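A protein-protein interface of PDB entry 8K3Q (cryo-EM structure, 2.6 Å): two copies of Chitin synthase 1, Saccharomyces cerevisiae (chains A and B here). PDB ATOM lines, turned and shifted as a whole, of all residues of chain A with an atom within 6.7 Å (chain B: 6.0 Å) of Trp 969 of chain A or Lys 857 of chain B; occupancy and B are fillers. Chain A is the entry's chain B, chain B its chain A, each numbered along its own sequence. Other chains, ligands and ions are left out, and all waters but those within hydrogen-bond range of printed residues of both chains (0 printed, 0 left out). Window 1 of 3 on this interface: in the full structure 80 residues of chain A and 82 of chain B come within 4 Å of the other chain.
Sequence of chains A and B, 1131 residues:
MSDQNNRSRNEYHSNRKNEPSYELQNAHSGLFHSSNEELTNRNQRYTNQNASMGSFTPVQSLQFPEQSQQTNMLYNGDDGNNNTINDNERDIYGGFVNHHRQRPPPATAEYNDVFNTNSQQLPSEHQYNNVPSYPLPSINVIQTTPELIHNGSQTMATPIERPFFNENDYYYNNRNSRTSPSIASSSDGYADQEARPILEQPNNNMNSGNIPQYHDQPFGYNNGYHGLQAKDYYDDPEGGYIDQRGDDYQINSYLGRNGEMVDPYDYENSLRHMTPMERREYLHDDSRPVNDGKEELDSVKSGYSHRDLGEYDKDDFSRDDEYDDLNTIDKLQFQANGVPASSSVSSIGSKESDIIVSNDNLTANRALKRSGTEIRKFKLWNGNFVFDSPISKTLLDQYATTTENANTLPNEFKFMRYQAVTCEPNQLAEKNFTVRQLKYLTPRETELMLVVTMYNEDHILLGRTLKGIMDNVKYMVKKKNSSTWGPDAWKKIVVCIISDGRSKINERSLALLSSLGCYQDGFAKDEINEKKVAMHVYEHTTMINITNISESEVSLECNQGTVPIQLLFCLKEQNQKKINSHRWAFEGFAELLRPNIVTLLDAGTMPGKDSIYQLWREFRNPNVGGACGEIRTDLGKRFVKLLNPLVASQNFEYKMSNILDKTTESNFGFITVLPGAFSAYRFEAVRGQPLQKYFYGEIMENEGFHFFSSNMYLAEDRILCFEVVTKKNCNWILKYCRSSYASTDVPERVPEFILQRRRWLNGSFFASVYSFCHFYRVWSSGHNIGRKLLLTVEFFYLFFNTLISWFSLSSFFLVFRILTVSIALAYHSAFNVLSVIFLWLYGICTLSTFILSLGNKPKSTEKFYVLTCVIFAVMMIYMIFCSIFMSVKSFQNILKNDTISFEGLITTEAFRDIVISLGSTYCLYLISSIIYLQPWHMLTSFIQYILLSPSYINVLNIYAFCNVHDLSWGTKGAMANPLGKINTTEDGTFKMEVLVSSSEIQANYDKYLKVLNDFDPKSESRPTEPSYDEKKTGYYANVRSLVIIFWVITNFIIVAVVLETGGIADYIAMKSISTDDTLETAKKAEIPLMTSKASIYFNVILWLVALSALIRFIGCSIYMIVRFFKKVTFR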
ATOM      1  N   LEU A 967     -25.771 -12.657  18.338  1.00  0.00           N
ATOM      2  CA  LEU A 967     -24.855 -13.246  19.301  1.00  0.00           C
ATOM      3  C   LEU A 967     -25.599 -14.030  20.375  1.00  0.00           C
ATOM      4  O   LEU A 967     -26.767 -13.779  20.679  1.00  0.00           O
ATOM      5  CB  LEU A 967     -23.997 -12.171  19.972  1.00  0.00           C
ATOM      6  N   SER A 968     -24.884 -14.991  20.960  1.00  0.00           N
ATOM      7  CA  SER A 968     -25.399 -15.801  22.062  1.00  0.00           C
ATOM      8  C   SER A 968     -24.205 -16.111  22.959  1.00  0.00           C
ATOM      9  O   SER A 968     -23.471 -17.070  22.708  1.00  0.00           O
ATOM     10  CB  SER A 968     -26.062 -17.075  21.555  1.00  0.00           C
ATOM     11  N   TRP A 969     -24.023 -15.300  23.998  1.00  0.00           N
ATOM     12  CA  TRP A 969     -22.830 -15.397  24.828  1.00  0.00           C
ATOM     13  C   TRP A 969     -22.823 -16.703  25.602  1.00  0.00           C
ATOM     14  O   TRP A 969     -21.960 -17.558  25.378  1.00  0.00           O
ATOM     15  CB  TRP A 969     -22.754 -14.211  25.790  1.00  0.00           C
ATOM     16  CG  TRP A 969     -22.347 -12.942  25.128  1.00  0.00           C
ATOM     17  CD1 TRP A 969     -23.159 -11.914  24.759  1.00  0.00           C
ATOM     18  CD2 TRP A 969     -21.022 -12.564  24.745  1.00  0.00           C
ATOM     19  NE1 TRP A 969     -22.423 -10.915  24.174  1.00  0.00           N
ATOM     20  CE2 TRP A 969     -21.107 -11.293  24.152  1.00  0.00           C
ATOM     21  CE3 TRP A 969     -19.772 -13.179  24.848  1.00  0.00           C
ATOM     22  CZ2 TRP A 969     -19.993 -10.623  23.666  1.00  0.00           C
ATOM     23  CZ3 TRP A 969     -18.667 -12.515  24.362  1.00  0.00           C
ATOM     24  CH2 TRP A 969     -18.783 -11.249  23.780  1.00  0.00           C
ATOM     25  N   GLU A1030     -17.027 -19.739  21.900  1.00  0.00           N
ATOM     26  CA  GLU A1030     -17.036 -18.429  22.540  1.00  0.00           C
ATOM     27  C   GLU A1030     -15.972 -17.488  21.991  1.00  0.00           C
ATOM     28  O   GLU A1030     -16.166 -16.270  22.035  1.00  0.00           O
ATOM     29  CB  GLU A1030     -16.909 -18.578  24.059  1.00  0.00           C
ATOM     30  CG  GLU A1030     -15.725 -19.382  24.546  1.00  0.00           C
ATOM     31  CD  GLU A1030     -16.073 -20.853  24.692  1.00  0.00           C
ATOM     32  OE1 GLU A1030     -17.081 -21.288  24.097  1.00  0.00           O
ATOM     33  OE2 GLU A1030     -15.366 -21.571  25.423  1.00  0.00           O
ATOM     34  N   THR A1033     -17.808 -16.140  19.125  1.00  0.00           N
ATOM     35  CA  THR A1033     -18.794 -15.201  19.650  1.00  0.00           C
ATOM     36  C   THR A1033     -18.163 -13.855  19.988  1.00  0.00           C
ATOM     37  O   THR A1033     -18.732 -12.800  19.693  1.00  0.00           O
ATOM     38  CB  THR A1033     -19.476 -15.805  20.875  1.00  0.00           C
ATOM     39  OG1 THR A1033     -20.201 -16.976  20.485  1.00  0.00           O
ATOM     40  CG2 THR A1033     -20.415 -14.822  21.526  1.00  0.00           C
ATOM     41  N   GLY A1034     -16.985 -13.871  20.608  1.00  0.00           N
ATOM     42  CA  GLY A1034     -16.302 -12.621  20.898  1.00  0.00           C
ATOM     43  C   GLY A1034     -15.918 -11.858  19.646  1.00  0.00           C
ATOM     44  O   GLY A1034     -16.053 -10.634  19.588  1.00  0.00           O
ATOM     45  N   TYR A1035     -15.433 -12.570  18.627  1.00  0.00           N
ATOM     46  CA  TYR A1035     -15.106 -11.900  17.371  1.00  0.00           C
ATOM     47  C   TYR A1035     -16.347 -11.288  16.737  1.00  0.00           C
ATOM     48  O   TYR A1035     -16.302 -10.168  16.214  1.00  0.00           O
ATOM     49  CB  TYR A1035     -14.443 -12.873  16.401  1.00  0.00           C
ATOM     50  CG  TYR A1035     -14.321 -12.328  15.000  1.00  0.00           C
ATOM     51  CD1 TYR A1035     -13.289 -11.471  14.662  1.00  0.00           C
ATOM     52  CD2 TYR A1035     -15.229 -12.674  14.014  1.00  0.00           C
ATOM     53  CE1 TYR A1035     -13.170 -10.968  13.393  1.00  0.00           C
ATOM     54  CE2 TYR A1035     -15.116 -12.171  12.740  1.00  0.00           C
ATOM     55  CZ  TYR A1035     -14.085 -11.318  12.436  1.00  0.00           C
ATOM     56  OH  TYR A1035     -13.960 -10.813  11.170  1.00  0.00           O
ATOM     57  N   ALA A1037     -19.110 -10.278  18.235  1.00  0.00           N
ATOM     58  CA  ALA A1037     -19.487  -9.090  18.989  1.00  0.00           C
ATOM     59  C   ALA A1037     -18.593  -7.897  18.687  1.00  0.00           C
ATOM     60  O   ALA A1037     -19.103  -6.782  18.512  1.00  0.00           O
ATOM     61  CB  ALA A1037     -19.457  -9.389  20.484  1.00  0.00           C
ATOM     62  N   ASN A1038     -17.280  -8.108  18.605  1.00  0.00           N
ATOM     63  CA  ASN A1038     -16.372  -7.017  18.278  1.00  0.00           C
ATOM     64  C   ASN A1038     -16.685  -6.432  16.914  1.00  0.00           C
ATOM     65  O   ASN A1038     -16.782  -5.208  16.758  1.00  0.00           O
ATOM     66  CB  ASN A1038     -14.928  -7.511  18.306  1.00  0.00           C
ATOM     67  CG  ASN A1038     -14.322  -7.455  19.673  1.00  0.00           C
ATOM     68  OD1 ASN A1038     -14.928  -6.951  20.612  1.00  0.00           O
ATOM     69  ND2 ASN A1038     -13.113  -7.968  19.799  1.00  0.00           N
ATOM     70  N   ARG A1040     -19.554  -6.650  15.338  1.00  0.00           N
ATOM     71  CA  ARG A1040     -20.866  -6.015  15.234  1.00  0.00           C
ATOM     72  C   ARG A1040     -20.858  -4.623  15.853  1.00  0.00           C
ATOM     73  O   ARG A1040     -21.542  -3.721  15.361  1.00  0.00           O
ATOM     74  CB  ARG A1040     -21.991  -6.838  15.878  1.00  0.00           C
ATOM     75  CG  ARG A1040     -22.804  -6.010  16.883  1.00  0.00           C
ATOM     76  CD  ARG A1040     -23.210  -6.662  18.196  1.00  0.00           C
ATOM     77  NE  ARG A1040     -24.141  -7.779  18.051  1.00  0.00           N
ATOM     78  CZ  ARG A1040     -25.190  -7.959  18.849  1.00  0.00           C
ATOM     79  NH1 ARG A1040     -25.419  -7.093  19.846  1.00  0.00           N
ATOM     80  NH2 ARG A1040     -26.046  -8.972  18.668  1.00  0.00           N
ATOM     81  N   LEU B 852     -20.319  -0.371  23.675  1.00  0.00           N
ATOM     82  CA  LEU B 852     -19.621  -1.563  24.128  1.00  0.00           C
ATOM     83  C   LEU B 852     -20.180  -2.121  25.422  1.00  0.00           C
ATOM     84  O   LEU B 852     -20.091  -3.329  25.644  1.00  0.00           O
ATOM     85  CB  LEU B 852     -18.135  -1.275  24.316  1.00  0.00           C
ATOM     86  CG  LEU B 852     -17.310  -1.054  23.057  1.00  0.00           C
ATOM     87  CD1 LEU B 852     -15.906  -0.743  23.442  1.00  0.00           C
ATOM     88  CD2 LEU B 852     -17.350  -2.270  22.183  1.00  0.00           C
ATOM     89  N   GLY B 855     -23.581  -3.877  24.411  1.00  0.00           N
ATOM     90  CA  GLY B 855     -23.516  -4.988  23.486  1.00  0.00           C
ATOM     91  C   GLY B 855     -22.418  -6.007  23.694  1.00  0.00           C
ATOM     92  O   GLY B 855     -22.564  -7.161  23.289  1.00  0.00           O
ATOM     93  N   ASN B 856     -21.309  -5.605  24.290  1.00  0.00           N
ATOM     94  CA  ASN B 856     -20.120  -6.434  24.327  1.00  0.00           C
ATOM     95  C   ASN B 856     -19.715  -6.688  25.782  1.00  0.00           C
ATOM     96  O   ASN B 856     -20.398  -6.268  26.719  1.00  0.00           O
ATOM     97  CB  ASN B 856     -19.047  -5.745  23.484  1.00  0.00           C
ATOM     98  CG  ASN B 856     -17.905  -6.646  23.140  1.00  0.00           C
ATOM     99  OD1 ASN B 856     -17.841  -7.786  23.586  1.00  0.00           O
ATOM    100  ND2 ASN B 856     -17.007  -6.157  22.302  1.00  0.00           N
ATOM    101  N   LYS B 857     -18.600  -7.392  25.987  1.00  0.00           N
ATOM    102  CA  LYS B 857     -18.133  -7.704  27.331  1.00  0.00           C
ATOM    103  C   LYS B 857     -16.773  -7.067  27.592  1.00  0.00           C
ATOM    104  O   LYS B 857     -15.933  -7.007  26.692  1.00  0.00           O
ATOM    105  CB  LYS B 857     -18.027  -9.218  27.550  1.00  0.00           C
ATOM    106  CG  LYS B 857     -19.318  -9.970  27.327  1.00  0.00           C
ATOM    107  CD  LYS B 857     -20.207  -9.916  28.550  1.00  0.00           C
ATOM    108  CE  LYS B 857     -21.666 -10.065  28.164  1.00  0.00           C
ATOM    109  NZ  LYS B 857     -22.578  -9.754  29.295  1.00  0.00           N
ATOM    110  N   PRO B 858     -16.526  -6.592  28.817  1.00  0.00           N
ATOM    111  CA  PRO B 858     -15.277  -5.858  29.082  1.00  0.00           C
ATOM    112  C   PRO B 858     -14.023  -6.684  28.876  1.00  0.00           C
ATOM    113  O   PRO B 858     -12.971  -6.114  28.571  1.00  0.00           O
ATOM    114  CB  PRO B 858     -15.425  -5.428  30.547  1.00  0.00           C
ATOM    115  CG  PRO B 858     -16.863  -5.516  30.832  1.00  0.00           C
ATOM    116  CD  PRO B 858     -17.392  -6.634  30.002  1.00  0.00           C
ATOM    117  N   LYS B 859     -14.093  -8.002  29.057  1.00  0.00           N
ATOM    118  CA  LYS B 859     -12.932  -8.847  28.813  1.00  0.00           C
ATOM    119  C   LYS B 859     -12.479  -8.765  27.363  1.00  0.00           C
ATOM    120  O   LYS B 859     -11.277  -8.816  27.083  1.00  0.00           O
ATOM    121  CB  LYS B 859     -13.260 -10.295  29.167  1.00  0.00           C
ATOM    122  CG  LYS B 859     -13.631 -10.535  30.618  1.00  0.00           C
ATOM    123  CD  LYS B 859     -12.472 -10.316  31.569  1.00  0.00           C
ATOM    124  CE  LYS B 859     -12.896 -10.650  32.992  1.00  0.00           C
ATOM    125  NZ  LYS B 859     -11.815 -10.414  33.986  1.00  0.00           N
ATOM    126  N   SER B 860     -13.429  -8.645  26.434  1.00  0.00           N
ATOM    127  CA  SER B 860     -13.108  -8.683  25.013  1.00  0.00           C
ATOM    128  C   SER B 860     -12.316  -7.458  24.577  1.00  0.00           C
ATOM    129  O   SER B 860     -11.409  -7.565  23.746  1.00  0.00           O
ATOM    130  CB  SER B 860     -14.392  -8.801  24.196  1.00  0.00           C
ATOM    131  OG  SER B 860     -15.040 -10.033  24.444  1.00  0.00           O
ATOM    132  N   THR B 861     -12.648  -6.287  25.107  1.00  0.00           N
ATOM    133  CA  THR B 861     -12.026  -5.033  24.694  1.00  0.00           C
ATOM    134  C   THR B 861     -11.368  -4.388  25.906  1.00  0.00           C
ATOM    135  O   THR B 861     -11.956  -3.519  26.546  1.00  0.00           O
ATOM    136  CB  THR B 861     -13.058  -4.102  24.074  1.00  0.00           C
ATOM    137  OG1 THR B 861     -14.043  -3.766  25.056  1.00  0.00           O
ATOM    138  CG2 THR B 861     -13.746  -4.770  22.904  1.00  0.00           C
ATOM    139  N   TYR B 865     -10.631   0.148  26.781  1.00  0.00           N
ATOM    140  CA  TYR B 865     -10.950   0.713  28.087  1.00  0.00           C
ATOM    141  C   TYR B 865      -9.738   1.388  28.712  1.00  0.00           C
ATOM    142  O   TYR B 865      -9.856   2.466  29.306  1.00  0.00           O
ATOM    143  CB  TYR B 865     -11.508  -0.369  29.000  1.00  0.00           C
ATOM    144  CG  TYR B 865     -12.969  -0.634  28.762  1.00  0.00           C
ATOM    145  CD1 TYR B 865     -13.875   0.406  28.700  1.00  0.00           C
ATOM    146  CD2 TYR B 865     -13.440  -1.919  28.581  1.00  0.00           C
ATOM    147  CE1 TYR B 865     -15.209   0.171  28.476  1.00  0.00           C
ATOM    148  CE2 TYR B 865     -14.769  -2.161  28.352  1.00  0.00           C
ATOM    149  CZ  TYR B 865     -15.649  -1.114  28.304  1.00  0.00           C
ATOM    150  OH  TYR B 865     -16.979  -1.351  28.081  1.00  0.00           O
ATOM    151  N   TYR B 959     -21.313   1.702  32.470  1.00  0.00           N
ATOM    152  CA  TYR B 959     -21.391   0.248  32.458  1.00  0.00           C
ATOM    153  C   TYR B 959     -22.334  -0.269  33.536  1.00  0.00           C
ATOM    154  O   TYR B 959     -23.046  -1.253  33.321  1.00  0.00           O
ATOM    155  CB  TYR B 959     -20.003  -0.364  32.626  1.00  0.00           C
ATOM    156  CG  TYR B 959     -20.013  -1.865  32.492  1.00  0.00           C
ATOM    157  CD1 TYR B 959     -20.161  -2.683  33.596  1.00  0.00           C
ATOM    158  CD2 TYR B 959     -19.896  -2.461  31.252  1.00  0.00           C
ATOM    159  CE1 TYR B 959     -20.181  -4.046  33.469  1.00  0.00           C
ATOM    160  CE2 TYR B 959     -19.919  -3.820  31.116  1.00  0.00           C
ATOM    161  CZ  TYR B 959     -20.061  -4.609  32.226  1.00  0.00           C
ATOM    162  OH  TYR B 959     -20.080  -5.974  32.086  1.00  0.00           O
ATOM    163  N   ASN B 963     -25.962  -2.400  32.566  1.00  0.00           N
ATOM    164  CA  ASN B 963     -25.950  -3.813  32.929  1.00  0.00           C
ATOM    165  C   ASN B 963     -26.623  -4.024  34.273  1.00  0.00           C
ATOM    166  O   ASN B 963     -26.094  -4.692  35.156  1.00  0.00           O
ATOM    167  CB  ASN B 963     -24.530  -4.359  32.979  1.00  0.00           C
ATOM    168  CG  ASN B 963     -23.862  -4.362  31.634  1.00  0.00           C
ATOM    169  OD1 ASN B 963     -23.790  -3.342  30.961  1.00  0.00           O
ATOM    170  ND2 ASN B 963     -23.374  -5.518  31.226  1.00  0.00           N
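No position is printed for both chains.
The side-chain amide nitrogen of Asn 856 of chain B is in hydrogen-bond range of the side-chain amide oxygen of Asn 1038 of chain A (2.8 Å).
Gly 855 of chain B touches Trp 969 of chain A.
CZ2 of Trp 969 of chain A touches OD1 of Asn 856 of chain B (3.6 Å).
Trp 969 of chain A touches Lys 857 of chain B (CZ2 to CG, 3.8 Å).
OG of Ser 860 of chain B touches CH2 of Trp 969 of chain A (3.99 Å).
CB of Ala 1037 of chain A touches OD1 of Asn 856 of chain B, at 3.8 Å.
Asn 1038 of chain A touches Thr 861 of chain B.
Along chain B the printed residues that touch a printed residue of chain A span positions 855 to 861.
Of the 10 printed residues of chain A, 3 touch a printed residue of chain B.
Printed residues of chain A that touch a printed residue of chain B: Trp 969, Ala 1037 and Asn 1038.
Among the printed residues, no Asp or Glu carboxylate lies within 4 Å of a Lys or Arg side-chain nitrogen of the other chain.
Printed residues of chain B within 4 Å of Trp 969 of chain A: Gly 855 (3.9 Å), Asn 856 (3.6 Å), Lys 857 (3.8 Å) and Ser 860 (3.99 Å).
Gly 1034 of chain A touches none of the printed residues of chain B.
Of the printed residues of chain B, Ala 1037 of chain A touches Asn 856 (3.8 Å).
Of the printed residues of chain A, Gly 855 of chain B touches Trp 969 (3.9 Å).
Lys 857 of chain B touches just one residue of chain A: Trp 969 (3.8 Å).
Of the printed residues of chain A, Thr 861 of chain B touches Asn 1038 (3.4 Å).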
